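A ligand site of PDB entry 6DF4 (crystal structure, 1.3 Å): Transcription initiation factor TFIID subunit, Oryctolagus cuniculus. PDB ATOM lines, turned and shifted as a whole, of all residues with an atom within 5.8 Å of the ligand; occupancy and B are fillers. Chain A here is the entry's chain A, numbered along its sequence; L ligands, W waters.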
ATOM      1  N   TRP A  55      -1.228   7.794  14.811  1.00  0.00           N
ATOM      2  CA  TRP A  55      -0.354   7.696  16.003  1.00  0.00           C
ATOM      3  C   TRP A  55       1.133   7.485  15.699  1.00  0.00           C
ATOM      4  O   TRP A  55       1.940   8.006  16.489  1.00  0.00           O
ATOM      5  CB  TRP A  55      -0.847   6.609  16.984  1.00  0.00           C
ATOM      6  CG  TRP A  55      -0.833   5.210  16.438  1.00  0.00           C
ATOM      7  CD1 TRP A  55      -1.867   4.595  15.766  1.00  0.00           C
ATOM      8  CD2 TRP A  55       0.301   4.338  16.311  1.00  0.00           C
ATOM      9  NE1 TRP A  55      -1.441   3.394  15.260  1.00  0.00           N
ATOM     10  CE2 TRP A  55      -0.115   3.202  15.576  1.00  0.00           C
ATOM     11  CE3 TRP A  55       1.646   4.404  16.744  1.00  0.00           C
ATOM     12  CZ2 TRP A  55       0.770   2.188  15.213  1.00  0.00           C
ATOM     13  CZ3 TRP A  55       2.500   3.370  16.430  1.00  0.00           C
ATOM     14  CH2 TRP A  55       2.063   2.282  15.652  1.00  0.00           C
ATOM     15  N   PRO A  56       1.591   6.781  14.636  1.00  0.00           N
ATOM     16  CA  PRO A  56       3.049   6.627  14.467  1.00  0.00           C
ATOM     17  C   PRO A  56       3.766   7.947  14.294  1.00  0.00           C
ATOM     18  O   PRO A  56       4.959   8.033  14.559  1.00  0.00           O
ATOM     19  CB  PRO A  56       3.177   5.795  13.193  1.00  0.00           C
ATOM     20  CG  PRO A  56       1.861   5.038  13.086  1.00  0.00           C
ATOM     21  CD  PRO A  56       0.854   6.048  13.581  1.00  0.00           C
ATOM     22  N   PHE A  57       3.041   8.989  13.841  1.00  0.00           N
ATOM     23  CA  PHE A  57       3.631  10.289  13.473  1.00  0.00           C
ATOM     24  C   PHE A  57       3.411  11.336  14.552  1.00  0.00           C
ATOM     25  O   PHE A  57       3.860  12.476  14.362  1.00  0.00           O
ATOM     26  CB  PHE A  57       2.992  10.743  12.154  1.00  0.00           C
ATOM     27  CG  PHE A  57       3.183   9.717  11.076  1.00  0.00           C
ATOM     28  CD1 PHE A  57       4.399   9.595  10.419  1.00  0.00           C
ATOM     29  CD2 PHE A  57       2.150   8.852  10.726  1.00  0.00           C
ATOM     30  CE1 PHE A  57       4.598   8.624   9.466  1.00  0.00           C
ATOM     31  CE2 PHE A  57       2.340   7.890   9.738  1.00  0.00           C
ATOM     32  CZ  PHE A  57       3.557   7.783   9.115  1.00  0.00           C
ATOM     33  N   HIS A  58       2.769  10.990  15.662  1.00  0.00           N
ATOM     34  CA  HIS A  58       2.436  11.997  16.679  1.00  0.00           C
ATOM     35  C   HIS A  58       3.591  12.451  17.518  1.00  0.00           C
ATOM     36  O   HIS A  58       3.478  13.493  18.164  1.00  0.00           O
ATOM     37  CB  HIS A  58       1.317  11.525  17.601  1.00  0.00           C
ATOM     38  CG  HIS A  58      -0.032  11.388  16.934  1.00  0.00           C
ATOM     39  ND1 HIS A  58      -1.124  10.919  17.657  1.00  0.00           N
ATOM     40  CD2 HIS A  58      -0.415  11.557  15.651  1.00  0.00           C
ATOM     41  CE1 HIS A  58      -2.136  10.890  16.804  1.00  0.00           C
ATOM     42  NE2 HIS A  58      -1.772  11.300  15.598  1.00  0.00           N
ATOM     43  N   HIS A  59       4.677  11.669  17.626  1.00  0.00           N
ATOM     44  CA  HIS A  59       5.801  11.929  18.534  1.00  0.00           C
ATOM     45  C   HIS A  59       7.065  11.437  17.857  1.00  0.00           C
ATOM     46  O   HIS A  59       6.993  10.557  16.980  1.00  0.00           O
ATOM     47  CB  HIS A  59       5.600  11.125  19.869  1.00  0.00           C
ATOM     48  CG  HIS A  59       4.346  11.465  20.607  1.00  0.00           C
ATOM     49  ND1 HIS A  59       4.196  12.677  21.278  1.00  0.00           N
ATOM     50  CD2 HIS A  59       3.175  10.775  20.694  1.00  0.00           C
ATOM     51  CE1 HIS A  59       2.969  12.674  21.790  1.00  0.00           C
ATOM     52  NE2 HIS A  59       2.314  11.546  21.469  1.00  0.00           N
ATOM     53  N   PRO A  60       8.248  11.924  18.291  1.00  0.00           N
ATOM     54  CA  PRO A  60       9.494  11.373  17.733  1.00  0.00           C
ATOM     55  C   PRO A  60       9.642   9.892  18.025  1.00  0.00           C
ATOM     56  O   PRO A  60       9.268   9.405  19.103  1.00  0.00           O
ATOM     57  CB  PRO A  60      10.617  12.160  18.438  1.00  0.00           C
ATOM     58  CG  PRO A  60       9.964  12.998  19.473  1.00  0.00           C
ATOM     59  CD  PRO A  60       8.468  12.961  19.331  1.00  0.00           C
ATOM     60  N   VAL A  61      10.267   9.178  17.092  1.00  0.00           N
ATOM     61  CA  VAL A  61      10.520   7.744  17.258  1.00  0.00           C
ATOM     62  C   VAL A  61      11.473   7.510  18.412  1.00  0.00           C
ATOM     63  O   VAL A  61      12.491   8.199  18.547  1.00  0.00           O
ATOM     64  CB  VAL A  61      11.125   7.169  15.951  1.00  0.00           C
ATOM     65  CG1 VAL A  61      11.530   5.703  16.127  1.00  0.00           C
ATOM     66  CG2 VAL A  61      10.158   7.318  14.801  1.00  0.00           C
ATOM     67  N   ASN A  62      11.154   6.521  19.243  1.00  0.00           N
ATOM     68  CA  ASN A  62      12.034   6.101  20.312  1.00  0.00           C
ATOM     69  C   ASN A  62      12.843   4.922  19.788  1.00  0.00           C
ATOM     70  O   ASN A  62      12.251   3.895  19.420  1.00  0.00           O
ATOM     71  CB  ASN A  62      11.161   5.682  21.502  1.00  0.00           C
ATOM     72  CG  ASN A  62      11.914   5.352  22.760  1.00  0.00           C
ATOM     73  OD1 ASN A  62      13.078   4.932  22.737  1.00  0.00           O
ATOM     74  ND2 ASN A  62      11.209   5.490  23.891  1.00  0.00           N
ATOM     75  N   LYS A  63      14.169   5.021  19.769  1.00  0.00           N
ATOM     76  CA  LYS A  63      15.006   3.912  19.288  1.00  0.00           C
ATOM     77  C   LYS A  63      14.831   2.628  20.100  1.00  0.00           C
ATOM     78  O   LYS A  63      15.130   1.556  19.581  1.00  0.00           O
ATOM     79  CB  LYS A  63      16.487   4.340  19.239  1.00  0.00           C
ATOM     80  CG  LYS A  63      17.057   4.714  20.588  1.00  0.00           C
ATOM     81  CD  LYS A  63      18.161   3.733  20.957  1.00  0.00           C
ATOM     82  CE  LYS A  63      18.973   4.220  22.119  1.00  0.00           C
ATOM     83  NZ  LYS A  63      20.222   3.419  22.275  1.00  0.00           N
ATOM     84  N   PHE A  65      12.022   1.391  20.696  1.00  0.00           N
ATOM     85  CA  PHE A  65      10.837   0.789  20.065  1.00  0.00           C
ATOM     86  C   PHE A  65      11.027   0.486  18.592  1.00  0.00           C
ATOM     87  O   PHE A  65      10.303  -0.358  18.040  1.00  0.00           O
ATOM     88  CB  PHE A  65       9.628   1.701  20.272  1.00  0.00           C
ATOM     89  CG  PHE A  65       9.290   2.066  21.705  1.00  0.00           C
ATOM     90  CD1 PHE A  65       9.697   1.261  22.768  1.00  0.00           C
ATOM     91  CD2 PHE A  65       8.487   3.156  21.988  1.00  0.00           C
ATOM     92  CE1 PHE A  65       9.360   1.595  24.094  1.00  0.00           C
ATOM     93  CE2 PHE A  65       8.157   3.491  23.293  1.00  0.00           C
ATOM     94  CZ  PHE A  65       8.572   2.696  24.340  1.00  0.00           C
ATOM     95  N   VAL A  66      11.923   1.235  17.906  1.00  0.00           N
ATOM     96  CA  VAL A  66      12.185   1.048  16.462  1.00  0.00           C
ATOM     97  C   VAL A  66      13.721   1.127  16.321  1.00  0.00           C
ATOM     98  O   VAL A  66      14.289   2.190  16.036  1.00  0.00           O
ATOM     99  CB  VAL A  66      11.474   2.066  15.560  1.00  0.00           C
ATOM    100  CG1 VAL A  66      11.644   1.660  14.102  1.00  0.00           C
ATOM    101  CG2 VAL A  66       9.965   2.216  15.905  1.00  0.00           C
ATOM    102  N   TYR A  69      15.628   2.862  13.249  1.00  0.00           N
ATOM    103  CA  TYR A  69      15.077   4.062  12.644  1.00  0.00           C
ATOM    104  C   TYR A  69      16.112   5.130  12.279  1.00  0.00           C
ATOM    105  O   TYR A  69      16.140   5.625  11.153  1.00  0.00           O
ATOM    106  CB  TYR A  69      13.969   4.660  13.530  1.00  0.00           C
ATOM    107  CG  TYR A  69      13.173   5.702  12.794  1.00  0.00           C
ATOM    108  CD1 TYR A  69      12.228   5.335  11.849  1.00  0.00           C
ATOM    109  CD2 TYR A  69      13.418   7.062  12.978  1.00  0.00           C
ATOM    110  CE1 TYR A  69      11.484   6.289  11.170  1.00  0.00           C
ATOM    111  CE2 TYR A  69      12.720   8.028  12.263  1.00  0.00           C
ATOM    112  CZ  TYR A  69      11.759   7.628  11.353  1.00  0.00           C
ATOM    113  OH  TYR A  69      11.004   8.552  10.663  1.00  0.00           O
ATOM    114  N   MET A  77      11.416  13.863  11.719  1.00  0.00           N
ATOM    115  CA  MET A  77      10.359  14.843  11.947  1.00  0.00           C
ATOM    116  C   MET A  77       9.110  14.178  12.455  1.00  0.00           C
ATOM    117  O   MET A  77       8.849  13.028  12.131  1.00  0.00           O
ATOM    118  CB  MET A  77      10.112  15.655  10.671  1.00  0.00           C
ATOM    119  CG  MET A  77       9.158  16.879  10.832  1.00  0.00           C
ATOM    120  SD  MET A  77       9.573  18.020  12.186  1.00  0.00           S
ATOM    121  CE  MET A  77      11.330  18.451  11.807  1.00  0.00           C
ATOM    122  N   ASP A  78       8.282  14.891  13.234  1.00  0.00           N
ATOM    123  CA  ASP A  78       7.027  14.322  13.736  1.00  0.00           C
ATOM    124  C   ASP A  78       6.106  15.498  14.058  1.00  0.00           C
ATOM    125  O   ASP A  78       6.546  16.666  14.095  1.00  0.00           O
ATOM    126  CB  ASP A  78       7.296  13.432  14.949  1.00  0.00           C
ATOM    127  CG  ASP A  78       7.803  14.264  16.089  1.00  0.00           C
ATOM    128  OD1 ASP A  78       9.026  14.499  16.145  1.00  0.00           O
ATOM    129  OD2 ASP A  78       6.947  14.790  16.866  1.00  0.00           O
ATOM    130  N   LEU A  79       4.842  15.211  14.340  1.00  0.00           N
ATOM    131  CA  LEU A  79       3.875  16.264  14.590  1.00  0.00           C
ATOM    132  C   LEU A  79       4.082  17.008  15.908  1.00  0.00           C
ATOM    133  O   LEU A  79       3.762  18.224  15.966  1.00  0.00           O
ATOM    134  CB  LEU A  79       2.460  15.724  14.461  1.00  0.00           C
ATOM    135  CG  LEU A  79       2.081  15.123  13.081  1.00  0.00           C
ATOM    136  CD1 LEU A  79       0.699  14.569  13.096  1.00  0.00           C
ATOM    137  CD2 LEU A  79       2.178  16.157  11.956  1.00  0.00           C
ATOM    138  N   ILE A 104       8.019  14.550   6.816  1.00  0.00           N
ATOM    139  CA  ILE A 104       7.402  13.353   7.399  1.00  0.00           C
ATOM    140  C   ILE A 104       7.085  12.344   6.283  1.00  0.00           C
ATOM    141  O   ILE A 104       7.376  11.136   6.405  1.00  0.00           O
ATOM    142  CB  ILE A 104       6.147  13.742   8.192  1.00  0.00           C
ATOM    143  CG1 ILE A 104       6.557  14.604   9.408  1.00  0.00           C
ATOM    144  CG2 ILE A 104       5.397  12.480   8.637  1.00  0.00           C
ATOM    145  CD1 ILE A 104       5.389  15.157  10.265  1.00  0.00           C
ATOM    146  N   SER A 108       8.856   8.604   5.617  1.00  0.00           N
ATOM    147  CA  SER A 108       8.148   7.324   5.567  1.00  0.00           C
ATOM    148  C   SER A 108       8.439   6.584   4.233  1.00  0.00           C
ATOM    149  O   SER A 108       8.597   5.358   4.235  1.00  0.00           O
ATOM    150  CB  SER A 108       6.654   7.555   5.718  1.00  0.00           C
ATOM    151  OG  SER A 108       5.960   6.314   5.799  1.00  0.00           O
ATOM    152  N   TYR A 111      11.922   5.016   4.861  1.00  0.00           N
ATOM    153  CA  TYR A 111      12.003   3.960   5.864  1.00  0.00           C
ATOM    154  C   TYR A 111      11.098   2.771   5.621  1.00  0.00           C
ATOM    155  O   TYR A 111      11.499   1.612   5.847  1.00  0.00           O
ATOM    156  CB  TYR A 111      11.725   4.528   7.273  1.00  0.00           C
ATOM    157  CG  TYR A 111      12.176   3.571   8.361  1.00  0.00           C
ATOM    158  CD1 TYR A 111      13.517   3.399   8.645  1.00  0.00           C
ATOM    159  CD2 TYR A 111      11.251   2.809   9.065  1.00  0.00           C
ATOM    160  CE1 TYR A 111      13.946   2.453   9.555  1.00  0.00           C
ATOM    161  CE2 TYR A 111      11.674   1.868  10.025  1.00  0.00           C
ATOM    162  CZ  TYR A 111      13.024   1.705  10.255  1.00  0.00           C
ATOM    163  OH  TYR A 111      13.517   0.808  11.187  1.00  0.00           O
ATOM    164  N   ASN A 112       9.885   3.041   5.165  1.00  0.00           N
ATOM    165  CA  ASN A 112       8.843   2.030   5.022  1.00  0.00           C
ATOM    166  C   ASN A 112       8.579   1.604   3.575  1.00  0.00           C
ATOM    167  O   ASN A 112       8.021   0.513   3.358  1.00  0.00           O
ATOM    168  CB  ASN A 112       7.538   2.574   5.625  1.00  0.00           C
ATOM    169  CG  ASN A 112       7.712   2.961   7.071  1.00  0.00           C
ATOM    170  OD1 ASN A 112       8.160   2.131   7.885  1.00  0.00           O
ATOM    171  ND2 ASN A 112       7.425   4.199   7.409  1.00  0.00           N
ATOM    172  N   TYR A 118       2.163   2.708   6.466  1.00  0.00           N
ATOM    173  CA  TYR A 118       2.665   3.914   7.170  1.00  0.00           C
ATOM    174  C   TYR A 118       2.722   5.092   6.190  1.00  0.00           C
ATOM    175  O   TYR A 118       2.339   6.213   6.540  1.00  0.00           O
ATOM    176  CB  TYR A 118       4.076   3.702   7.723  1.00  0.00           C
ATOM    177  CG  TYR A 118       4.172   2.831   8.947  1.00  0.00           C
ATOM    178  CD1 TYR A 118       3.680   3.260  10.176  1.00  0.00           C
ATOM    179  CD2 TYR A 118       4.785   1.581   8.896  1.00  0.00           C
ATOM    180  CE1 TYR A 118       3.825   2.481  11.328  1.00  0.00           C
ATOM    181  CE2 TYR A 118       4.913   0.787  10.031  1.00  0.00           C
ATOM    182  CZ  TYR A 118       4.435   1.242  11.257  1.00  0.00           C
ATOM    183  OH  TYR A 118       4.513   0.442  12.379  1.00  0.00           O
HETATM  184  C1  LIG L   1       6.677   6.986  11.881  1.00  0.00           C
HETATM  185  C2  LIG L   1       7.382   4.741  11.141  1.00  0.00           C
HETATM  186  C3  LIG L   1       6.681   5.101  13.429  1.00  0.00           C
HETATM  187  C4  LIG L   1       6.920   3.814  13.818  1.00  0.00           C
HETATM  188  C5  LIG L   1       7.370   2.877  12.771  1.00  0.00           C
HETATM  189  C6  LIG L   1       7.733   1.493  12.765  1.00  0.00           C
HETATM  190  C7  LIG L   1       8.104   1.213  11.488  1.00  0.00           C
HETATM  191  C8  LIG L   1       7.593   3.384  11.488  1.00  0.00           C
HETATM  192  C9  LIG L   1       7.774   7.852  12.511  1.00  0.00           C
HETATM  193  C10 LIG L   1       5.242   5.447  19.300  1.00  0.00           C
HETATM  194  C11 LIG L   1       6.480   2.645  17.924  1.00  0.00           C
HETATM  195  C12 LIG L   1       6.054   1.775  16.934  1.00  0.00           C
HETATM  196  C13 LIG L   1       7.399  10.218  13.156  1.00  0.00           C
HETATM  197  N1  LIG L   1       6.922   5.557  12.135  1.00  0.00           N
HETATM  198  C14 LIG L   1       7.604   9.321  12.215  1.00  0.00           C
HETATM  199  O1  LIG L   1       8.796   4.950  18.738  1.00  0.00           O
HETATM  200  C15 LIG L   1       6.731   3.417  15.234  1.00  0.00           C
HETATM  201  N2  LIG L   1       6.726   5.478  19.471  1.00  0.00           N
HETATM  202  O2  LIG L   1       7.634   5.181   9.993  1.00  0.00           O
HETATM  203  C16 LIG L   1       4.805   6.891  19.022  1.00  0.00           C
HETATM  204  C17 LIG L   1       7.231   6.373  20.524  1.00  0.00           C
HETATM  205  C18 LIG L   1       7.044   3.904  17.583  1.00  0.00           C
HETATM  206  C19 LIG L   1       6.182   2.166  15.600  1.00  0.00           C
HETATM  207  N3  LIG L   1       8.030   2.345  10.711  1.00  0.00           N
HETATM  208  C20 LIG L   1       6.681   7.775  20.245  1.00  0.00           C
HETATM  209  C21 LIG L   1       7.564   4.816  18.627  1.00  0.00           C
HETATM  210  O3  LIG L   1       5.252   7.745  20.098  1.00  0.00           O
HETATM  211  C22 LIG L   1       7.169   4.265  16.241  1.00  0.00           C
HETATM  212  O   HOH W   1       1.627   8.136  19.282  1.00  0.00           O
HETATM  213  O   HOH W   2       7.034   7.720  16.448  1.00  0.00           O
HETATM  214  O   HOH W   3       8.827   9.985  21.754  1.00  0.00           O
HETATM  215  O   HOH W   4       8.990   7.421   8.900  1.00  0.00           O
HETATM  216  O   HOH W   5       4.448   7.934  22.762  1.00  0.00           O
HETATM  217  O   HOH W   6       7.748   9.878   8.818  1.00  0.00           O
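O2 of the ligand is in hydrogen-bond range of ND2 of Asn 112 (2.8 Å).
N of Asn 62 lies within hydrogen-bond range of O1 of the ligand (2.9 Å).
The side-chain amide nitrogen (ND2) of Asn 112 is in hydrogen-bond range of the side-chain hydroxyl (OG) of Ser 108 (3.0 Å).
The backbone NH (N) of Leu 79 is in hydrogen-bond range of the backbone carbonyl oxygen (O) of Phe 57, 2.9 Å away.
CZ3 of Trp 55 touches C12 of the ligand, 3.9 Å away.
Pro 56 touches the ligand.
CE1 of Phe 57 touches C1 of the ligand, 3.6 Å away.
His 59 touches the ligand (CB to O3, 3.4 Å).
Pro 60 touches the ligand (O to C20, 3.3 Å).
Val 61 touches the ligand.
Phe 65 touches the ligand (CB to O1, 3.7 Å).
Val 66 touches the ligand.
OH of Tyr 69 touches C9 of the ligand, at 3.8 Å.
Met 77 touches the ligand.
Asp 78 touches the ligand.
Tyr 111 touches the ligand.
OH of Tyr 118 touches C6 of the ligand (3.4 Å).
The nearest printed residue that does not touch the ligand is Ser 108 (4.7 Å).
Water W4 lies within hydrogen-bond range of an oxygen (O2) of the ligand, the side-chain hydroxyl of Tyr 69 and the backbone NH of Ser 108.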
